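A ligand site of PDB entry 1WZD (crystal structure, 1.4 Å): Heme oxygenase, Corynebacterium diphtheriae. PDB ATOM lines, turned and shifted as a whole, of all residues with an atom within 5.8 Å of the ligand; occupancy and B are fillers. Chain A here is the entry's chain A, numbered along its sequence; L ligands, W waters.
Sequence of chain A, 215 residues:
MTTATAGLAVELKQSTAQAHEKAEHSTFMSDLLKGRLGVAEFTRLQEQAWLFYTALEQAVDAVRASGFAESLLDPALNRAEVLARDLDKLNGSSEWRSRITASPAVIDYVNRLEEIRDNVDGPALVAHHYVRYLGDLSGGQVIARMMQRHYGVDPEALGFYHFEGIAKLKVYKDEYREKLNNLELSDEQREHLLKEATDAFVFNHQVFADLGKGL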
ATOM      1  N   ALA A   9       1.911   6.897 -28.290  1.00  0.00           N
ATOM      2  CA  ALA A   9       1.893   8.257 -27.761  1.00  0.00           C
ATOM      3  C   ALA A   9       1.225   8.285 -26.380  1.00  0.00           C
ATOM      4  O   ALA A   9       1.782   8.830 -25.430  1.00  0.00           O
ATOM      5  CB  ALA A   9       1.199   9.204 -28.725  1.00  0.00           C
ATOM      6  N   LEU A  12       3.397   6.283 -23.802  1.00  0.00           N
ATOM      7  CA  LEU A  12       4.538   7.122 -23.436  1.00  0.00           C
ATOM      8  C   LEU A  12       4.174   8.154 -22.381  1.00  0.00           C
ATOM      9  O   LEU A  12       4.870   8.285 -21.377  1.00  0.00           O
ATOM     10  CB  LEU A  12       5.096   7.848 -24.650  1.00  0.00           C
ATOM     11  CG  LEU A  12       6.330   7.268 -25.342  1.00  0.00           C
ATOM     12  CD1 LEU A  12       6.575   7.978 -26.670  1.00  0.00           C
ATOM     13  CD2 LEU A  12       7.554   7.339 -24.420  1.00  0.00           C
ATOM     14  N   LYS A  13       3.077   8.867 -22.611  1.00  0.00           N
ATOM     15  CA  LYS A  13       2.655   9.911 -21.676  1.00  0.00           C
ATOM     16  C   LYS A  13       2.328   9.313 -20.310  1.00  0.00           C
ATOM     17  O   LYS A  13       2.694   9.880 -19.273  1.00  0.00           O
ATOM     18  CB  LYS A  13       1.456  10.699 -22.231  1.00  0.00           C
ATOM     19  CG  LYS A  13       1.157  11.991 -21.480  1.00  0.00           C
ATOM     20  CD  LYS A  13       0.201  12.876 -22.278  1.00  0.00           C
ATOM     21  CE  LYS A  13      -0.068  14.196 -21.548  1.00  0.00           C
ATOM     22  NZ  LYS A  13      -1.003  15.088 -22.285  1.00  0.00           N
ATOM     23  N   HIS A  20       8.426  12.493 -15.254  1.00  0.00           N
ATOM     24  CA  HIS A  20       8.134  13.784 -15.848  1.00  0.00           C
ATOM     25  C   HIS A  20       7.761  14.818 -14.788  1.00  0.00           C
ATOM     26  O   HIS A  20       8.349  15.901 -14.745  1.00  0.00           O
ATOM     27  CB  HIS A  20       6.998  13.645 -16.880  1.00  0.00           C
ATOM     28  CG  HIS A  20       6.770  14.875 -17.706  1.00  0.00           C
ATOM     29  ND1 HIS A  20       5.864  14.899 -18.741  1.00  0.00           N
ATOM     30  CD2 HIS A  20       7.337  16.100 -17.654  1.00  0.00           C
ATOM     31  CE1 HIS A  20       5.873  16.110 -19.291  1.00  0.00           C
ATOM     32  NE2 HIS A  20       6.753  16.849 -18.650  1.00  0.00           N
ATOM     33  N   ALA A  23      10.770  15.859 -12.692  1.00  0.00           N
ATOM     34  CA  ALA A  23      11.727  16.719 -13.402  1.00  0.00           C
ATOM     35  C   ALA A  23      11.184  18.143 -13.534  1.00  0.00           C
ATOM     36  O   ALA A  23      11.867  19.111 -13.252  1.00  0.00           O
ATOM     37  CB  ALA A  23      12.036  16.144 -14.773  1.00  0.00           C
ATOM     38  N   GLU A  24       9.918  18.236 -13.955  1.00  0.00           N
ATOM     39  CA  GLU A  24       9.273  19.515 -14.201  1.00  0.00           C
ATOM     40  C   GLU A  24       9.156  20.350 -12.929  1.00  0.00           C
ATOM     41  O   GLU A  24       9.289  21.578 -12.970  1.00  0.00           O
ATOM     42  CB  GLU A  24       7.890  19.254 -14.808  1.00  0.00           C
ATOM     43  CG  GLU A  24       7.408  20.318 -15.745  1.00  0.00           C
ATOM     44  CD  GLU A  24       6.146  19.919 -16.457  1.00  0.00           C
ATOM     45  OE1 GLU A  24       5.057  20.258 -15.959  1.00  0.00           O
ATOM     46  OE2 GLU A  24       6.232  19.247 -17.502  1.00  0.00           O
ATOM     47  N   LEU A  33      10.962  29.636 -12.808  1.00  0.00           N
ATOM     48  CA  LEU A  33       9.691  30.039 -13.400  1.00  0.00           C
ATOM     49  C   LEU A  33       8.878  30.993 -12.521  1.00  0.00           C
ATOM     50  O   LEU A  33       7.993  31.685 -13.023  1.00  0.00           O
ATOM     51  CB  LEU A  33       8.856  28.813 -13.801  1.00  0.00           C
ATOM     52  CG  LEU A  33       9.492  27.941 -14.889  1.00  0.00           C
ATOM     53  CD1 LEU A  33       8.679  26.689 -15.144  1.00  0.00           C
ATOM     54  CD2 LEU A  33       9.687  28.721 -16.190  1.00  0.00           C
ATOM     55  N   TYR A 130      11.486  12.545 -28.078  1.00  0.00           N
ATOM     56  CA  TYR A 130      10.201  12.864 -27.460  1.00  0.00           C
ATOM     57  C   TYR A 130      10.383  13.766 -26.238  1.00  0.00           C
ATOM     58  O   TYR A 130       9.734  14.812 -26.138  1.00  0.00           O
ATOM     59  CB  TYR A 130       9.514  11.556 -27.077  1.00  0.00           C
ATOM     60  CG  TYR A 130       8.305  11.673 -26.174  1.00  0.00           C
ATOM     61  CD1 TYR A 130       7.054  11.997 -26.693  1.00  0.00           C
ATOM     62  CD2 TYR A 130       8.416  11.399 -24.812  1.00  0.00           C
ATOM     63  CE1 TYR A 130       5.936  12.070 -25.861  1.00  0.00           C
ATOM     64  CE2 TYR A 130       7.303  11.479 -23.974  1.00  0.00           C
ATOM     65  CZ  TYR A 130       6.067  11.806 -24.509  1.00  0.00           C
ATOM     66  OH  TYR A 130       4.967  11.875 -23.685  1.00  0.00           O
ATOM     67  N   VAL A 131      11.243  13.355 -25.323  1.00  0.00           N
ATOM     68  CA  VAL A 131      11.429  14.078 -24.057  1.00  0.00           C
ATOM     69  C   VAL A 131      11.887  15.519 -24.296  1.00  0.00           C
ATOM     70  O   VAL A 131      11.341  16.454 -23.716  1.00  0.00           O
ATOM     71  CB  VAL A 131      12.338  13.307 -23.064  1.00  0.00           C
ATOM     72  CG1 VAL A 131      12.701  14.179 -21.878  1.00  0.00           C
ATOM     73  CG2 VAL A 131      11.646  12.026 -22.591  1.00  0.00           C
ATOM     74  N   ARG A 132      12.878  15.692 -25.173  1.00  0.00           N
ATOM     75  CA  ARG A 132      13.391  17.027 -25.437  1.00  0.00           C
ATOM     76  C   ARG A 132      12.521  17.829 -26.391  1.00  0.00           C
ATOM     77  O   ARG A 132      12.000  18.864 -26.008  1.00  0.00           O
ATOM     78  CB  ARG A 132      14.870  17.003 -25.893  1.00  0.00           C
ATOM     79  CG  ARG A 132      15.925  16.764 -24.784  1.00  0.00           C
ATOM     80  CD  ARG A 132      15.674  17.541 -23.479  1.00  0.00           C
ATOM     81  NE  ARG A 132      15.388  18.951 -23.708  1.00  0.00           N
ATOM     82  CZ  ARG A 132      15.368  19.901 -22.771  1.00  0.00           C
ATOM     83  NH1 ARG A 132      15.681  19.602 -21.518  1.00  0.00           N
ATOM     84  NH2 ARG A 132      15.061  21.144 -23.100  1.00  0.00           N
ATOM     85  N   LEU A 134       9.484  17.301 -28.048  1.00  0.00           N
ATOM     86  CA  LEU A 134       8.057  17.478 -27.785  1.00  0.00           C
ATOM     87  C   LEU A 134       7.875  18.361 -26.549  1.00  0.00           C
ATOM     88  O   LEU A 134       6.948  19.157 -26.481  1.00  0.00           O
ATOM     89  CB  LEU A 134       7.280  16.159 -27.689  1.00  0.00           C
ATOM     90  CG  LEU A 134       5.757  16.281 -27.862  1.00  0.00           C
ATOM     91  CD1 LEU A 134       5.388  17.008 -29.147  1.00  0.00           C
ATOM     92  CD2 LEU A 134       5.064  14.928 -27.810  1.00  0.00           C
ATOM     93  N   GLY A 135       8.780  18.232 -25.582  1.00  0.00           N
ATOM     94  CA  GLY A 135       8.816  19.151 -24.452  1.00  0.00           C
ATOM     95  C   GLY A 135       9.001  20.594 -24.873  1.00  0.00           C
ATOM     96  O   GLY A 135       8.261  21.481 -24.427  1.00  0.00           O
ATOM     97  N   ASP A 136       9.975  20.836 -25.746  1.00  0.00           N
ATOM     98  CA  ASP A 136      10.248  22.177 -26.239  1.00  0.00           C
ATOM     99  C   ASP A 136       9.038  22.756 -26.972  1.00  0.00           C
ATOM    100  O   ASP A 136       8.700  23.917 -26.783  1.00  0.00           O
ATOM    101  CB  ASP A 136      11.446  22.175 -27.194  1.00  0.00           C
ATOM    102  CG  ASP A 136      12.754  21.769 -26.525  1.00  0.00           C
ATOM    103  OD1 ASP A 136      13.635  21.335 -27.280  1.00  0.00           O
ATOM    104  OD2 ASP A 136      12.901  21.885 -25.290  1.00  0.00           O
ATOM    105  N   SER A 138       5.917  21.831 -26.647  1.00  0.00           N
ATOM    106  CA  SER A 138       4.766  21.915 -25.750  1.00  0.00           C
ATOM    107  C   SER A 138       4.853  23.090 -24.793  1.00  0.00           C
ATOM    108  O   SER A 138       3.892  23.852 -24.662  1.00  0.00           O
ATOM    109  CB  SER A 138       4.639  20.633 -24.949  1.00  0.00           C
ATOM    110  OG  SER A 138       4.321  19.539 -25.788  1.00  0.00           O
ATOM    111  N   GLY A 139       5.993  23.223 -24.111  1.00  0.00           N
ATOM    112  CA  GLY A 139       6.146  24.223 -23.059  1.00  0.00           C
ATOM    113  C   GLY A 139       7.006  25.412 -23.407  1.00  0.00           C
ATOM    114  O   GLY A 139       7.151  26.316 -22.577  1.00  0.00           O
ATOM    115  N   GLY A 140       7.547  25.455 -24.620  1.00  0.00           N
ATOM    116  CA  GLY A 140       8.524  26.489 -24.985  1.00  0.00           C
ATOM    117  C   GLY A 140       8.007  27.900 -24.854  1.00  0.00           C
ATOM    118  O   GLY A 140       8.728  28.778 -24.366  1.00  0.00           O
ATOM    119  N   VAL A 142       5.610  28.975 -22.910  1.00  0.00           N
ATOM    120  CA  VAL A 142       5.458  29.255 -21.480  1.00  0.00           C
ATOM    121  C   VAL A 142       6.791  29.678 -20.864  1.00  0.00           C
ATOM    122  O   VAL A 142       6.872  30.715 -20.218  1.00  0.00           O
ATOM    123  CB  VAL A 142       4.867  28.042 -20.722  1.00  0.00           C
ATOM    124  CG1 VAL A 142       4.949  28.251 -19.205  1.00  0.00           C
ATOM    125  CG2 VAL A 142       3.420  27.812 -21.130  1.00  0.00           C
ATOM    126  N   ILE A 143       7.835  28.880 -21.085  1.00  0.00           N
ATOM    127  CA  ILE A 143       9.136  29.164 -20.492  1.00  0.00           C
ATOM    128  C   ILE A 143       9.693  30.482 -21.023  1.00  0.00           C
ATOM    129  O   ILE A 143      10.160  31.326 -20.253  1.00  0.00           O
ATOM    130  CB  ILE A 143      10.117  27.988 -20.715  1.00  0.00           C
ATOM    131  CG1 ILE A 143       9.563  26.750 -20.008  1.00  0.00           C
ATOM    132  CG2 ILE A 143      11.511  28.357 -20.203  1.00  0.00           C
ATOM    133  CD1 ILE A 143      10.218  25.436 -20.383  1.00  0.00           C
ATOM    134  N   ARG A 177       2.702  13.182 -32.564  1.00  0.00           N
ATOM    135  CA  ARG A 177       2.140  12.079 -31.799  1.00  0.00           C
ATOM    136  C   ARG A 177       1.611  10.966 -32.709  1.00  0.00           C
ATOM    137  O   ARG A 177       1.759   9.776 -32.402  1.00  0.00           O
ATOM    138  CB  ARG A 177       1.084  12.568 -30.805  1.00  0.00           C
ATOM    139  CG  ARG A 177       1.703  13.176 -29.536  1.00  0.00           C
ATOM    140  CD  ARG A 177       0.665  13.676 -28.534  1.00  0.00           C
ATOM    141  NE  ARG A 177       0.016  14.892 -29.010  1.00  0.00           N
ATOM    142  CZ  ARG A 177       0.276  16.134 -28.577  1.00  0.00           C
ATOM    143  NH1 ARG A 177       1.187  16.342 -27.637  1.00  0.00           N
ATOM    144  NH2 ARG A 177      -0.378  17.162 -29.091  1.00  0.00           N
ATOM    145  N   PHE A 201      13.799  11.533 -18.760  1.00  0.00           N
ATOM    146  CA  PHE A 201      13.259  12.495 -17.794  1.00  0.00           C
ATOM    147  C   PHE A 201      14.127  12.569 -16.538  1.00  0.00           C
ATOM    148  O   PHE A 201      14.384  13.664 -16.023  1.00  0.00           O
ATOM    149  CB  PHE A 201      11.814  12.175 -17.433  1.00  0.00           C
ATOM    150  CG  PHE A 201      10.803  12.679 -18.418  1.00  0.00           C
ATOM    151  CD1 PHE A 201      10.032  11.789 -19.159  1.00  0.00           C
ATOM    152  CD2 PHE A 201      10.601  14.045 -18.596  1.00  0.00           C
ATOM    153  CE1 PHE A 201       9.077  12.257 -20.063  1.00  0.00           C
ATOM    154  CE2 PHE A 201       9.644  14.521 -19.506  1.00  0.00           C
ATOM    155  CZ  PHE A 201       8.894  13.613 -20.243  1.00  0.00           C
ATOM    156  N   ASN A 204      17.256  14.621 -17.084  1.00  0.00           N
ATOM    157  CA  ASN A 204      16.945  16.041 -17.071  1.00  0.00           C
ATOM    158  C   ASN A 204      16.679  16.596 -15.674  1.00  0.00           C
ATOM    159  O   ASN A 204      17.096  17.707 -15.348  1.00  0.00           O
ATOM    160  CB  ASN A 204      15.786  16.331 -18.024  1.00  0.00           C
ATOM    161  CG  ASN A 204      16.255  16.435 -19.451  1.00  0.00           C
ATOM    162  OD1 ASN A 204      16.751  17.483 -19.870  1.00  0.00           O
ATOM    163  ND2 ASN A 204      16.130  15.344 -20.205  1.00  0.00           N
ATOM    164  N   HIS A 205      15.989  15.817 -14.856  1.00  0.00           N
ATOM    165  CA  HIS A 205      15.809  16.139 -13.433  1.00  0.00           C
ATOM    166  C   HIS A 205      17.165  16.372 -12.775  1.00  0.00           C
ATOM    167  O   HIS A 205      17.347  17.350 -12.039  1.00  0.00           O
ATOM    168  CB  HIS A 205      15.088  14.961 -12.768  1.00  0.00           C
ATOM    169  CG  HIS A 205      14.581  15.238 -11.383  1.00  0.00           C
ATOM    170  ND1 HIS A 205      14.945  16.339 -10.637  1.00  0.00           N
ATOM    171  CD2 HIS A 205      13.725  14.519 -10.606  1.00  0.00           C
ATOM    172  CE1 HIS A 205      14.339  16.278  -9.456  1.00  0.00           C
ATOM    173  NE2 HIS A 205      13.594  15.187  -9.421  1.00  0.00           N
ATOM    174  N   PHE A 208      18.796  19.680 -13.684  1.00  0.00           N
ATOM    175  CA  PHE A 208      18.225  20.761 -12.879  1.00  0.00           C
ATOM    176  C   PHE A 208      18.799  20.737 -11.458  1.00  0.00           C
ATOM    177  O   PHE A 208      19.128  21.784 -10.894  1.00  0.00           O
ATOM    178  CB  PHE A 208      16.700  20.652 -12.793  1.00  0.00           C
ATOM    179  CG  PHE A 208      15.988  20.819 -14.099  1.00  0.00           C
ATOM    180  CD1 PHE A 208      16.425  21.720 -15.064  1.00  0.00           C
ATOM    181  CD2 PHE A 208      14.821  20.101 -14.344  1.00  0.00           C
ATOM    182  CE1 PHE A 208      15.749  21.877 -16.270  1.00  0.00           C
ATOM    183  CE2 PHE A 208      14.124  20.248 -15.540  1.00  0.00           C
ATOM    184  CZ  PHE A 208      14.581  21.138 -16.507  1.00  0.00           C
HETATM  185  O1  LIG L   1       1.989  14.955 -25.310  1.00  0.00           O
HETATM  186  C1  LIG L   1       2.905  14.255 -24.720  1.00  0.00           C
HETATM  187  O2  LIG L   1       2.745  13.021 -24.618  1.00  0.00           O
HETATM  188  C2  LIG L   1       4.075  14.872 -24.197  1.00  0.00           C
HETATM  189  C3  LIG L   1       4.260  16.406 -24.385  1.00  0.00           C
HETATM  190  C4  LIG L   1       5.422  16.749 -23.483  1.00  0.00           C
HETATM  191  C5  LIG L   1       6.649  16.017 -23.531  1.00  0.00           C
HETATM  192  C6  LIG L   1       7.699  16.388 -22.660  1.00  0.00           C
HETATM  193  C7  LIG L   1       7.474  17.469 -21.781  1.00  0.00           C
HETATM  194  N1  LIG L   1       8.464  17.890 -20.870  1.00  0.00           N
HETATM  195 FE1  LIG L   1       7.577  18.910 -19.169  1.00  0.00          FE
HETATM  196  O3  LIG L   1       9.256  18.596 -18.213  1.00  0.00           O
HETATM  197  C8  LIG L   1      10.517  18.376 -18.673  1.00  0.00           C
HETATM  198  C9  LIG L   1      10.762  17.958 -20.037  1.00  0.00           C
HETATM  199  C10 LIG L   1      12.079  17.737 -20.454  1.00  0.00           C
HETATM  200  C11 LIG L   1      13.129  17.935 -19.574  1.00  0.00           C
HETATM  201  C12 LIG L   1      12.894  18.335 -18.248  1.00  0.00           C
HETATM  202  C13 LIG L   1      11.596  18.569 -17.777  1.00  0.00           C
HETATM  203  C14 LIG L   1       9.729  17.739 -20.989  1.00  0.00           C
HETATM  204  O4  LIG L   1       7.679  20.786 -19.087  1.00  0.00           O
HETATM  205  C15 LIG L   1       6.768  21.770 -19.341  1.00  0.00           C
HETATM  206  C16 LIG L   1       6.927  23.037 -18.691  1.00  0.00           C
HETATM  207  C17 LIG L   1       5.950  24.048 -18.976  1.00  0.00           C
HETATM  208  C18 LIG L   1       4.861  23.836 -19.860  1.00  0.00           C
HETATM  209  C19 LIG L   1       4.732  22.564 -20.494  1.00  0.00           C
HETATM  210  C20 LIG L   1       5.667  21.516 -20.253  1.00  0.00           C
HETATM  211  C21 LIG L   1       5.494  20.258 -20.935  1.00  0.00           C
HETATM  212  N2  LIG L   1       6.254  19.225 -20.798  1.00  0.00           N
HETATM  213  C22 LIG L   1       6.255  18.184 -21.754  1.00  0.00           C
HETATM  214  C23 LIG L   1       5.210  17.820 -22.619  1.00  0.00           C
HETATM  215  O   HOH W   1       1.496  11.506 -26.162  1.00  0.00           O
HETATM  216  O   HOH W   2       5.404  26.175 -16.485  1.00  0.00           O
HETATM  217  O   HOH W   3      11.977  19.620 -23.294  1.00  0.00           O
HETATM  218  O   HOH W   4       4.804  13.283 -21.472  1.00  0.00           O
HETATM  219  O   HOH W   5      -0.686  14.656 -24.995  1.00  0.00           O
HETATM  220  O   HOH W   6      10.069  21.572 -17.580  1.00  0.00           O
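NH1 of Arg 177 lies within salt-bridge range of O1 of the ligand, 2.8 Å away. An iron atom (FE1) of the ligand is bound by the side-chain carboxylate of Glu 24. NE2 of His 20 is bound to FE1 of the ligand (2.3 Å). OH of Tyr 130 lies within hydrogen-bond range of O2 of the ligand, at 2.7 Å.
Water W1 lies within hydrogen-bond range of an oxygen (O2) of the ligand (2.5 Å) and the backbone carbonyl oxygen of Ala 9 (2.8 Å). Water W5 bridges an oxygen (O1) of the ligand (2.7 Å) and the side-chain amino group of Lys 13 (2.8 Å). Water W4 lies within hydrogen-bond range of OH of Tyr 130 (2.6 Å) and ND1 of His 20 (3.3 Å).
Residues that only touch the ligand: Gly 139, Val 131, Gly 135, Ser 138, Lys 13, Asn 204, Phe 208, Phe 201, Arg 132, Leu 134 and Ala 23. Hydrophobic or aromatic side chains within 4 Å of the ligand: His 20, Ala 23, Tyr 130, Val 131, Leu 134, Phe 201 and Phe 208. Within 4 Å of the ligand: Lys 13, His 20, Ala 23, Glu 24, Tyr 130, Val 131, Arg 132, Leu 134, Gly 135, Ser 138, Gly 139, Arg 177, Phe 201, Asn 204 and Phe 208.
OD1 of Asn 204 sits at hydrogen-bond distance from NH1 of Arg 132, at 2.9 Å. The backbone carbonyl oxygen (O) of Leu 134 sits at hydrogen-bond distance from the side-chain hydroxyl (OG) of Ser 138, at 2.7 Å. OD2 of Asp 136 lies within salt-bridge range of NH2 of Arg 132, 3.2 Å away.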
